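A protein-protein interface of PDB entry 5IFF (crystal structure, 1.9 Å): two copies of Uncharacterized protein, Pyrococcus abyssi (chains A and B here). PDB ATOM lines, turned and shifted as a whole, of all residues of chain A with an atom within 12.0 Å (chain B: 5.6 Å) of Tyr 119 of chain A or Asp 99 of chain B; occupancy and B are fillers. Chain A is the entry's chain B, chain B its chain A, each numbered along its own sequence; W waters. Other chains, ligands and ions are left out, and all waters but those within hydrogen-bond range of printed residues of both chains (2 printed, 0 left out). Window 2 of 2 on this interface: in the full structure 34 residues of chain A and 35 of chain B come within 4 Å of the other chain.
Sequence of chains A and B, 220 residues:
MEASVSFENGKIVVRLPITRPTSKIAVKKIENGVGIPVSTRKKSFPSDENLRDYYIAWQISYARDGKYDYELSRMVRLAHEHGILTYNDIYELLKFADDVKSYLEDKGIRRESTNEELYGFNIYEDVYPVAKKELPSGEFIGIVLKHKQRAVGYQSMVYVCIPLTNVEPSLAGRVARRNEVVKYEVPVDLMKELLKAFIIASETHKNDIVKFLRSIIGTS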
ATOM      1  N   THR A 114      -8.254   3.034  25.295  1.00  0.00           N
ATOM      2  CA  THR A 114      -9.710   3.094  25.340  1.00  0.00           C
ATOM      3  C   THR A 114     -10.193   3.742  24.044  1.00  0.00           C
ATOM      4  O   THR A 114      -9.385   4.089  23.179  1.00  0.00           O
ATOM      5  CB  THR A 114     -10.227   3.904  26.538  1.00  0.00           C
ATOM      6  OG1 THR A 114     -10.078   5.304  26.263  1.00  0.00           O
ATOM      7  CG2 THR A 114      -9.464   3.566  27.792  1.00  0.00           C
ATOM      8  N   ASN A 115     -11.502   3.918  23.909  1.00  0.00           N
ATOM      9  CA  ASN A 115     -12.047   4.637  22.766  1.00  0.00           C
ATOM     10  C   ASN A 115     -12.527   6.038  23.169  1.00  0.00           C
ATOM     11  O   ASN A 115     -13.304   6.668  22.454  1.00  0.00           O
ATOM     12  CB  ASN A 115     -13.191   3.843  22.121  1.00  0.00           C
ATOM     13  CG  ASN A 115     -12.728   2.505  21.551  1.00  0.00           C
ATOM     14  OD1 ASN A 115     -11.534   2.294  21.323  1.00  0.00           O
ATOM     15  ND2 ASN A 115     -13.675   1.595  21.323  1.00  0.00           N
ATOM     16  N   GLU A 116     -12.052   6.521  24.309  1.00  0.00           N
ATOM     17  CA  GLU A 116     -12.471   7.814  24.826  1.00  0.00           C
ATOM     18  C   GLU A 116     -11.408   8.855  24.573  1.00  0.00           C
ATOM     19  O   GLU A 116     -10.225   8.546  24.535  1.00  0.00           O
ATOM     20  CB  GLU A 116     -12.741   7.749  26.331  1.00  0.00           C
ATOM     21  CG  GLU A 116     -14.145   7.351  26.740  1.00  0.00           C
ATOM     22  CD  GLU A 116     -14.351   7.463  28.246  1.00  0.00           C
ATOM     23  OE1 GLU A 116     -13.436   7.974  28.942  1.00  0.00           O
ATOM     24  OE2 GLU A 116     -15.426   7.040  28.731  1.00  0.00           O
ATOM     25  N   GLU A 117     -11.843  10.099  24.430  1.00  0.00           N
ATOM     26  CA  GLU A 117     -10.921  11.223  24.333  1.00  0.00           C
ATOM     27  C   GLU A 117     -11.378  12.295  25.299  1.00  0.00           C
ATOM     28  O   GLU A 117     -12.552  12.370  25.649  1.00  0.00           O
ATOM     29  CB  GLU A 117     -10.857  11.783  22.905  1.00  0.00           C
ATOM     30  CG  GLU A 117     -10.457  10.743  21.863  1.00  0.00           C
ATOM     31  CD  GLU A 117     -10.296  11.341  20.474  1.00  0.00           C
ATOM     32  OE1 GLU A 117     -10.420  12.573  20.353  1.00  0.00           O
ATOM     33  OE2 GLU A 117     -10.046  10.576  19.519  1.00  0.00           O
ATOM     34  N   LEU A 118     -10.435  13.120  25.714  1.00  0.00           N
ATOM     35  CA  LEU A 118     -10.721  14.307  26.490  1.00  0.00           C
ATOM     36  C   LEU A 118     -10.245  15.541  25.713  1.00  0.00           C
ATOM     37  O   LEU A 118      -9.044  15.808  25.644  1.00  0.00           O
ATOM     38  CB  LEU A 118     -10.049  14.212  27.847  1.00  0.00           C
ATOM     39  CG  LEU A 118     -10.149  15.410  28.768  1.00  0.00           C
ATOM     40  CD1 LEU A 118     -11.600  15.686  29.085  1.00  0.00           C
ATOM     41  CD2 LEU A 118      -9.339  15.158  30.047  1.00  0.00           C
ATOM     42  N   TYR A 119     -11.194  16.282  25.134  1.00  0.00           N
ATOM     43  CA  TYR A 119     -10.908  17.450  24.330  1.00  0.00           C
ATOM     44  C   TYR A 119      -9.722  17.210  23.384  1.00  0.00           C
ATOM     45  O   TYR A 119      -8.797  18.025  23.322  1.00  0.00           O
ATOM     46  CB  TYR A 119     -10.661  18.685  25.235  1.00  0.00           C
ATOM     47  CG  TYR A 119     -11.909  19.086  26.012  1.00  0.00           C
ATOM     48  CD1 TYR A 119     -12.979  19.715  25.367  1.00  0.00           C
ATOM     49  CD2 TYR A 119     -12.034  18.783  27.363  1.00  0.00           C
ATOM     50  CE1 TYR A 119     -14.125  20.051  26.041  1.00  0.00           C
ATOM     51  CE2 TYR A 119     -13.189  19.119  28.071  1.00  0.00           C
ATOM     52  CZ  TYR A 119     -14.228  19.759  27.398  1.00  0.00           C
ATOM     53  OH  TYR A 119     -15.370  20.094  28.073  1.00  0.00           O
ATOM     54  N   GLY A 120      -9.740  16.078  22.685  1.00  0.00           N
ATOM     55  CA  GLY A 120      -8.728  15.794  21.676  1.00  0.00           C
ATOM     56  C   GLY A 120      -7.565  14.929  22.126  1.00  0.00           C
ATOM     57  O   GLY A 120      -6.757  14.509  21.318  1.00  0.00           O
ATOM     58  N   PHE A 121      -7.459  14.682  23.423  1.00  0.00           N
ATOM     59  CA  PHE A 121      -6.398  13.858  23.950  1.00  0.00           C
ATOM     60  C   PHE A 121      -6.978  12.466  24.122  1.00  0.00           C
ATOM     61  O   PHE A 121      -8.030  12.309  24.723  1.00  0.00           O
ATOM     62  CB  PHE A 121      -5.878  14.388  25.298  1.00  0.00           C
ATOM     63  CG  PHE A 121      -5.025  15.628  25.193  1.00  0.00           C
ATOM     64  CD1 PHE A 121      -5.574  16.855  24.813  1.00  0.00           C
ATOM     65  CD2 PHE A 121      -3.678  15.582  25.500  1.00  0.00           C
ATOM     66  CE1 PHE A 121      -4.774  17.995  24.730  1.00  0.00           C
ATOM     67  CE2 PHE A 121      -2.874  16.721  25.451  1.00  0.00           C
ATOM     68  CZ  PHE A 121      -3.422  17.928  25.041  1.00  0.00           C
ATOM     69  N   ASN A 122      -6.309  11.458  23.595  1.00  0.00           N
ATOM     70  CA  ASN A 122      -6.730  10.086  23.839  1.00  0.00           C
ATOM     71  C   ASN A 122      -6.591   9.685  25.301  1.00  0.00           C
ATOM     72  O   ASN A 122      -5.586   9.997  25.937  1.00  0.00           O
ATOM     73  CB  ASN A 122      -5.911   9.152  22.964  1.00  0.00           C
ATOM     74  CG  ASN A 122      -6.132   9.412  21.488  1.00  0.00           C
ATOM     75  OD1 ASN A 122      -5.321  10.047  20.828  1.00  0.00           O
ATOM     76  ND2 ASN A 122      -7.261   8.949  20.973  1.00  0.00           N
ATOM     77  N   ILE A 123      -7.594   8.968  25.821  1.00  0.00           N
ATOM     78  CA  ILE A 123      -7.584   8.477  27.183  1.00  0.00           C
ATOM     79  C   ILE A 123      -7.123   7.027  27.231  1.00  0.00           C
ATOM     80  O   ILE A 123      -7.633   6.172  26.491  1.00  0.00           O
ATOM     81  CB  ILE A 123      -8.973   8.560  27.848  1.00  0.00           C
ATOM     82  CG1 ILE A 123      -9.418  10.021  28.015  1.00  0.00           C
ATOM     83  CG2 ILE A 123      -8.953   7.862  29.226  1.00  0.00           C
ATOM     84  CD1 ILE A 123      -8.537  10.832  28.941  1.00  0.00           C
ATOM     85  N   TYR A 124      -6.156   6.768  28.103  1.00  0.00           N
ATOM     86  CA  TYR A 124      -5.679   5.416  28.390  1.00  0.00           C
ATOM     87  C   TYR A 124      -5.932   5.131  29.867  1.00  0.00           C
ATOM     88  O   TYR A 124      -6.167   6.056  30.649  1.00  0.00           O
ATOM     89  CB  TYR A 124      -4.186   5.258  28.116  1.00  0.00           C
ATOM     90  CG  TYR A 124      -3.773   5.378  26.683  1.00  0.00           C
ATOM     91  CD1 TYR A 124      -3.728   6.622  26.044  1.00  0.00           C
ATOM     92  CD2 TYR A 124      -3.393   4.256  25.953  1.00  0.00           C
ATOM     93  CE1 TYR A 124      -3.327   6.742  24.709  1.00  0.00           C
ATOM     94  CE2 TYR A 124      -2.994   4.372  24.604  1.00  0.00           C
ATOM     95  CZ  TYR A 124      -2.964   5.615  24.009  1.00  0.00           C
ATOM     96  OH  TYR A 124      -2.570   5.748  22.712  1.00  0.00           O
ATOM     97  N   LEU B  94      -6.876  30.641  24.240  1.00  0.00           N
ATOM     98  CA  LEU B  94      -7.887  31.192  25.183  1.00  0.00           C
ATOM     99  C   LEU B  94      -9.291  30.700  24.823  1.00  0.00           C
ATOM    100  O   LEU B  94     -10.118  30.384  25.728  1.00  0.00           O
ATOM    101  CB  LEU B  94      -7.822  32.725  25.213  1.00  0.00           C
ATOM    102  CG  LEU B  94      -6.541  33.311  25.843  1.00  0.00           C
ATOM    103  CD1 LEU B  94      -6.564  34.847  25.665  1.00  0.00           C
ATOM    104  CD2 LEU B  94      -6.416  32.926  27.287  1.00  0.00           C
ATOM    105  N   LYS B  95      -9.569  30.623  23.528  1.00  0.00           N
ATOM    106  CA  LYS B  95     -10.838  30.080  23.028  1.00  0.00           C
ATOM    107  C   LYS B  95     -11.030  28.598  23.408  1.00  0.00           C
ATOM    108  O   LYS B  95     -12.129  28.164  23.753  1.00  0.00           O
ATOM    109  CB  LYS B  95     -10.923  30.195  21.513  1.00  0.00           C
ATOM    110  CG  LYS B  95     -12.338  29.941  20.971  1.00  0.00           C
ATOM    111  CD  LYS B  95     -12.466  30.301  19.471  1.00  0.00           C
ATOM    112  CE  LYS B  95     -11.714  31.587  19.096  1.00  0.00           C
ATOM    113  NZ  LYS B  95     -12.333  32.369  17.949  1.00  0.00           N
ATOM    114  N   PHE B  96      -9.969  27.827  23.263  1.00  0.00           N
ATOM    115  CA  PHE B  96      -9.977  26.421  23.689  1.00  0.00           C
ATOM    116  C   PHE B  96     -10.329  26.304  25.187  1.00  0.00           C
ATOM    117  O   PHE B  96     -11.249  25.548  25.571  1.00  0.00           O
ATOM    118  CB  PHE B  96      -8.615  25.781  23.393  1.00  0.00           C
ATOM    119  CG  PHE B  96      -8.475  24.355  23.901  1.00  0.00           C
ATOM    120  CD1 PHE B  96      -9.130  23.306  23.256  1.00  0.00           C
ATOM    121  CD2 PHE B  96      -7.694  24.083  25.011  1.00  0.00           C
ATOM    122  CE1 PHE B  96      -8.993  21.975  23.703  1.00  0.00           C
ATOM    123  CE2 PHE B  96      -7.553  22.758  25.477  1.00  0.00           C
ATOM    124  CZ  PHE B  96      -8.214  21.703  24.808  1.00  0.00           C
ATOM    125  N   ALA B  97      -9.629  27.074  26.018  1.00  0.00           N
ATOM    126  CA  ALA B  97      -9.898  27.053  27.444  1.00  0.00           C
ATOM    127  C   ALA B  97     -11.343  27.413  27.776  1.00  0.00           C
ATOM    128  O   ALA B  97     -11.896  26.863  28.740  1.00  0.00           O
ATOM    129  CB  ALA B  97      -8.940  27.971  28.179  1.00  0.00           C
ATOM    130  N   ASP B  98     -11.969  28.313  26.995  1.00  0.00           N
ATOM    131  CA  ASP B  98     -13.376  28.660  27.215  1.00  0.00           C
ATOM    132  C   ASP B  98     -14.289  27.471  27.028  1.00  0.00           C
ATOM    133  O   ASP B  98     -15.321  27.359  27.683  1.00  0.00           O
ATOM    134  CB  ASP B  98     -13.833  29.778  26.261  1.00  0.00           C
ATOM    135  CG  ASP B  98     -13.274  31.137  26.650  1.00  0.00           C
ATOM    136  OD1 ASP B  98     -12.899  31.282  27.841  1.00  0.00           O
ATOM    137  OD2 ASP B  98     -13.216  32.048  25.786  1.00  0.00           O
ATOM    138  N   ASP B  99     -13.917  26.611  26.099  1.00  0.00           N
ATOM    139  CA  ASP B  99     -14.717  25.441  25.732  1.00  0.00           C
ATOM    140  C   ASP B  99     -14.532  24.245  26.706  1.00  0.00           C
ATOM    141  O   ASP B  99     -15.339  23.345  26.758  1.00  0.00           O
ATOM    142  CB  ASP B  99     -14.366  24.991  24.296  1.00  0.00           C
ATOM    143  CG  ASP B  99     -14.584  26.102  23.234  1.00  0.00           C
ATOM    144  OD1 ASP B  99     -15.433  27.005  23.431  1.00  0.00           O
ATOM    145  OD2 ASP B  99     -13.905  26.058  22.181  1.00  0.00           O
ATOM    146  N   VAL B 100     -13.444  24.226  27.451  1.00  0.00           N
ATOM    147  CA  VAL B 100     -13.163  23.091  28.348  1.00  0.00           C
ATOM    148  C   VAL B 100     -13.968  23.220  29.659  1.00  0.00           C
ATOM    149  O   VAL B 100     -13.783  24.224  30.380  1.00  0.00           O
ATOM    150  CB  VAL B 100     -11.663  23.028  28.654  1.00  0.00           C
ATOM    151  CG1 VAL B 100     -11.344  21.938  29.715  1.00  0.00           C
ATOM    152  CG2 VAL B 100     -10.883  22.754  27.352  1.00  0.00           C
ATOM    153  N   LYS B 101     -14.822  22.234  29.975  1.00  0.00           N
ATOM    154  CA  LYS B 101     -15.655  22.241  31.211  1.00  0.00           C
ATOM    155  C   LYS B 101     -15.543  20.902  31.965  1.00  0.00           C
ATOM    156  O   LYS B 101     -16.316  20.603  32.870  1.00  0.00           O
ATOM    157  CB  LYS B 101     -17.128  22.500  30.888  1.00  0.00           C
ATOM    158  CG  LYS B 101     -17.435  23.790  30.145  1.00  0.00           C
ATOM    159  CD  LYS B 101     -17.228  25.008  31.024  1.00  0.00           C
ATOM    160  CE  LYS B 101     -17.491  26.286  30.261  1.00  0.00           C
ATOM    161  NZ  LYS B 101     -17.020  27.467  31.029  1.00  0.00           N
ATOM    162  N   SER B 102     -14.595  20.079  31.552  1.00  0.00           N
ATOM    163  CA  SER B 102     -14.377  18.795  32.213  1.00  0.00           C
ATOM    164  C   SER B 102     -12.885  18.481  32.166  1.00  0.00           C
ATOM    165  O   SER B 102     -12.203  18.876  31.223  1.00  0.00           O
ATOM    166  CB  SER B 102     -15.188  17.698  31.533  1.00  0.00           C
ATOM    167  OG  SER B 102     -14.889  16.469  32.140  1.00  0.00           O
ATOM    168  N   TYR B 103     -12.382  17.789  33.183  1.00  0.00           N
ATOM    169  CA  TYR B 103     -10.940  17.687  33.396  1.00  0.00           C
ATOM    170  C   TYR B 103     -10.523  16.275  33.712  1.00  0.00           C
ATOM    171  O   TYR B 103     -11.333  15.487  34.212  1.00  0.00           O
ATOM    172  CB  TYR B 103     -10.510  18.617  34.544  1.00  0.00           C
ATOM    173  CG  TYR B 103     -11.009  20.030  34.302  1.00  0.00           C
ATOM    174  CD1 TYR B 103     -10.315  20.892  33.465  1.00  0.00           C
ATOM    175  CD2 TYR B 103     -12.192  20.482  34.880  1.00  0.00           C
ATOM    176  CE1 TYR B 103     -10.807  22.209  33.197  1.00  0.00           C
ATOM    177  CE2 TYR B 103     -12.662  21.764  34.655  1.00  0.00           C
ATOM    178  CZ  TYR B 103     -11.956  22.625  33.811  1.00  0.00           C
ATOM    179  OH  TYR B 103     -12.421  23.897  33.542  1.00  0.00           O
ATOM    180  N   LYS B 133      -1.114  12.516  24.000  1.00  0.00           N
ATOM    181  CA  LYS B 133      -1.178  12.961  22.593  1.00  0.00           C
ATOM    182  C   LYS B 133       0.199  12.812  21.986  1.00  0.00           C
ATOM    183  O   LYS B 133       1.204  13.084  22.665  1.00  0.00           O
ATOM    184  CB  LYS B 133      -1.644  14.442  22.508  1.00  0.00           C
ATOM    185  CG  LYS B 133      -1.905  14.931  21.069  1.00  0.00           C
ATOM    186  CD  LYS B 133      -2.361  16.407  21.085  1.00  0.00           C
ATOM    187  CE  LYS B 133      -3.782  16.569  21.613  1.00  0.00           C
ATOM    188  NZ  LYS B 133      -4.426  17.842  21.105  1.00  0.00           N
ATOM    189  N   LYS B 196      -2.393  23.266  26.276  1.00  0.00           N
ATOM    190  CA  LYS B 196      -3.688  22.571  26.232  1.00  0.00           C
ATOM    191  C   LYS B 196      -3.755  21.434  27.235  1.00  0.00           C
ATOM    192  O   LYS B 196      -4.830  21.193  27.834  1.00  0.00           O
ATOM    193  CB  LYS B 196      -3.965  22.038  24.856  1.00  0.00           C
ATOM    194  CG  LYS B 196      -4.282  23.196  23.855  1.00  0.00           C
ATOM    195  CD  LYS B 196      -4.321  22.688  22.404  1.00  0.00           C
ATOM    196  CE  LYS B 196      -5.530  21.839  22.184  1.00  0.00           C
ATOM    197  NZ  LYS B 196      -5.859  21.801  20.725  1.00  0.00           N
ATOM    198  N   ILE B 200      -6.630  21.029  30.260  1.00  0.00           N
ATOM    199  CA  ILE B 200      -7.589  19.922  30.458  1.00  0.00           C
ATOM    200  C   ILE B 200      -7.257  19.069  31.714  1.00  0.00           C
ATOM    201  O   ILE B 200      -8.053  18.232  32.119  1.00  0.00           O
ATOM    202  CB  ILE B 200      -7.682  19.011  29.249  1.00  0.00           C
ATOM    203  CG1 ILE B 200      -6.367  18.248  29.018  1.00  0.00           C
ATOM    204  CG2 ILE B 200      -8.118  19.814  28.020  1.00  0.00           C
ATOM    205  CD1 ILE B 200      -6.570  16.975  28.168  1.00  0.00           C
HETATM  206  O   HOH W   1     -17.646  22.122  26.630  1.00  0.00           O
HETATM  207  O   HOH W   2      -6.952  18.543  21.732  1.00  0.00           O
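Among the printed residues, pairs that only touch across the chains: Tyr 119 of chain A with Ser 102 of chain B, Phe 121 of chain A with Ile 200 of chain B, Tyr 119 of chain A with Asp 99 of chain B, Phe 121 of chain A with Lys 133 of chain B, Tyr 119 of chain A with Val 100 of chain B, Gly 120 of chain A with Lys 133 of chain B, Leu 118 of chain A with Ile 200 of chain B, Leu 118 of chain A with Ser 102 of chain B, Tyr 119 of chain A with Phe 96 of chain B and Tyr 119 of chain A with Ile 200 of chain B.
The side-chain hydroxyl of Tyr 119 of chain A is in hydrogen-bond range of the backbone NH of Lys 101 of chain B (2.9 Å).
No position is printed for both chains. Of the 11 pairs that touch across the chains among the printed residues, none has its exchanged pair printed and touching as well.
Of the 13 printed residues of chain B, 7 touch a printed residue of chain A. Along chain B the printed residues that touch a printed residue of chain A span positions 96 to 200. Among the printed residues, 11 pairs touch across the chains.
OH of Tyr 103 of chain B lies within hydrogen-bond range of O of Val 100 of chain B, 3.5 Å away.
Tyr 119 of chain A touches just these residues of chain B: Phe 96, Asp 99, Val 100, Lys 101, Ser 102 and Ile 200. Asp 99 of chain B touches one residue of chain A. No residue of chain A comes within 4 Å of Lys 95 of chain B. No residue of chain A comes within 4 Å of Ala 97 of chain B. No residue of chain A comes within 4 Å of Asp 98 of chain B. Val 100 of chain B touches one residue of chain A. Lys 101 of chain B touches just one residue of chain A: Tyr 119. Ser 102 of chain B touches two residues of chain A. Of chain A, only Leu 118, Tyr 119 and Phe 121 come within 4 Å of Ile 200 of chain B. Of the printed residues of chain B, Gly 120 of chain A touches Lys 133. Of the printed residues of chain A, Lys 133 of chain B touches Gly 120 (3.6 Å) and Phe 121 (3.6 Å). Of the printed residues of chain B, Phe 121 of chain A touches Lys 133 (3.6 Å) and Ile 200 (3.5 Å). Printed residues of chain B within 4 Å of Leu 118 of chain A: Ser 102 and Ile 200. The nearest residue of chain A that does not touch Asp 99 of chain B is Leu 118 of chain A (8.8 Å). The nearest printed residue of chain B that does not touch Phe 121 of chain A is Lys 196 of chain B (4.1 Å).
Water W2 bridges O of Tyr 119 of chain A (2.5 Å) and NZ of Lys 133 of chain B (2.7 Å). Water W1 bridges O of Asp 99 of chain B and OH of Tyr 119 of chain A.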
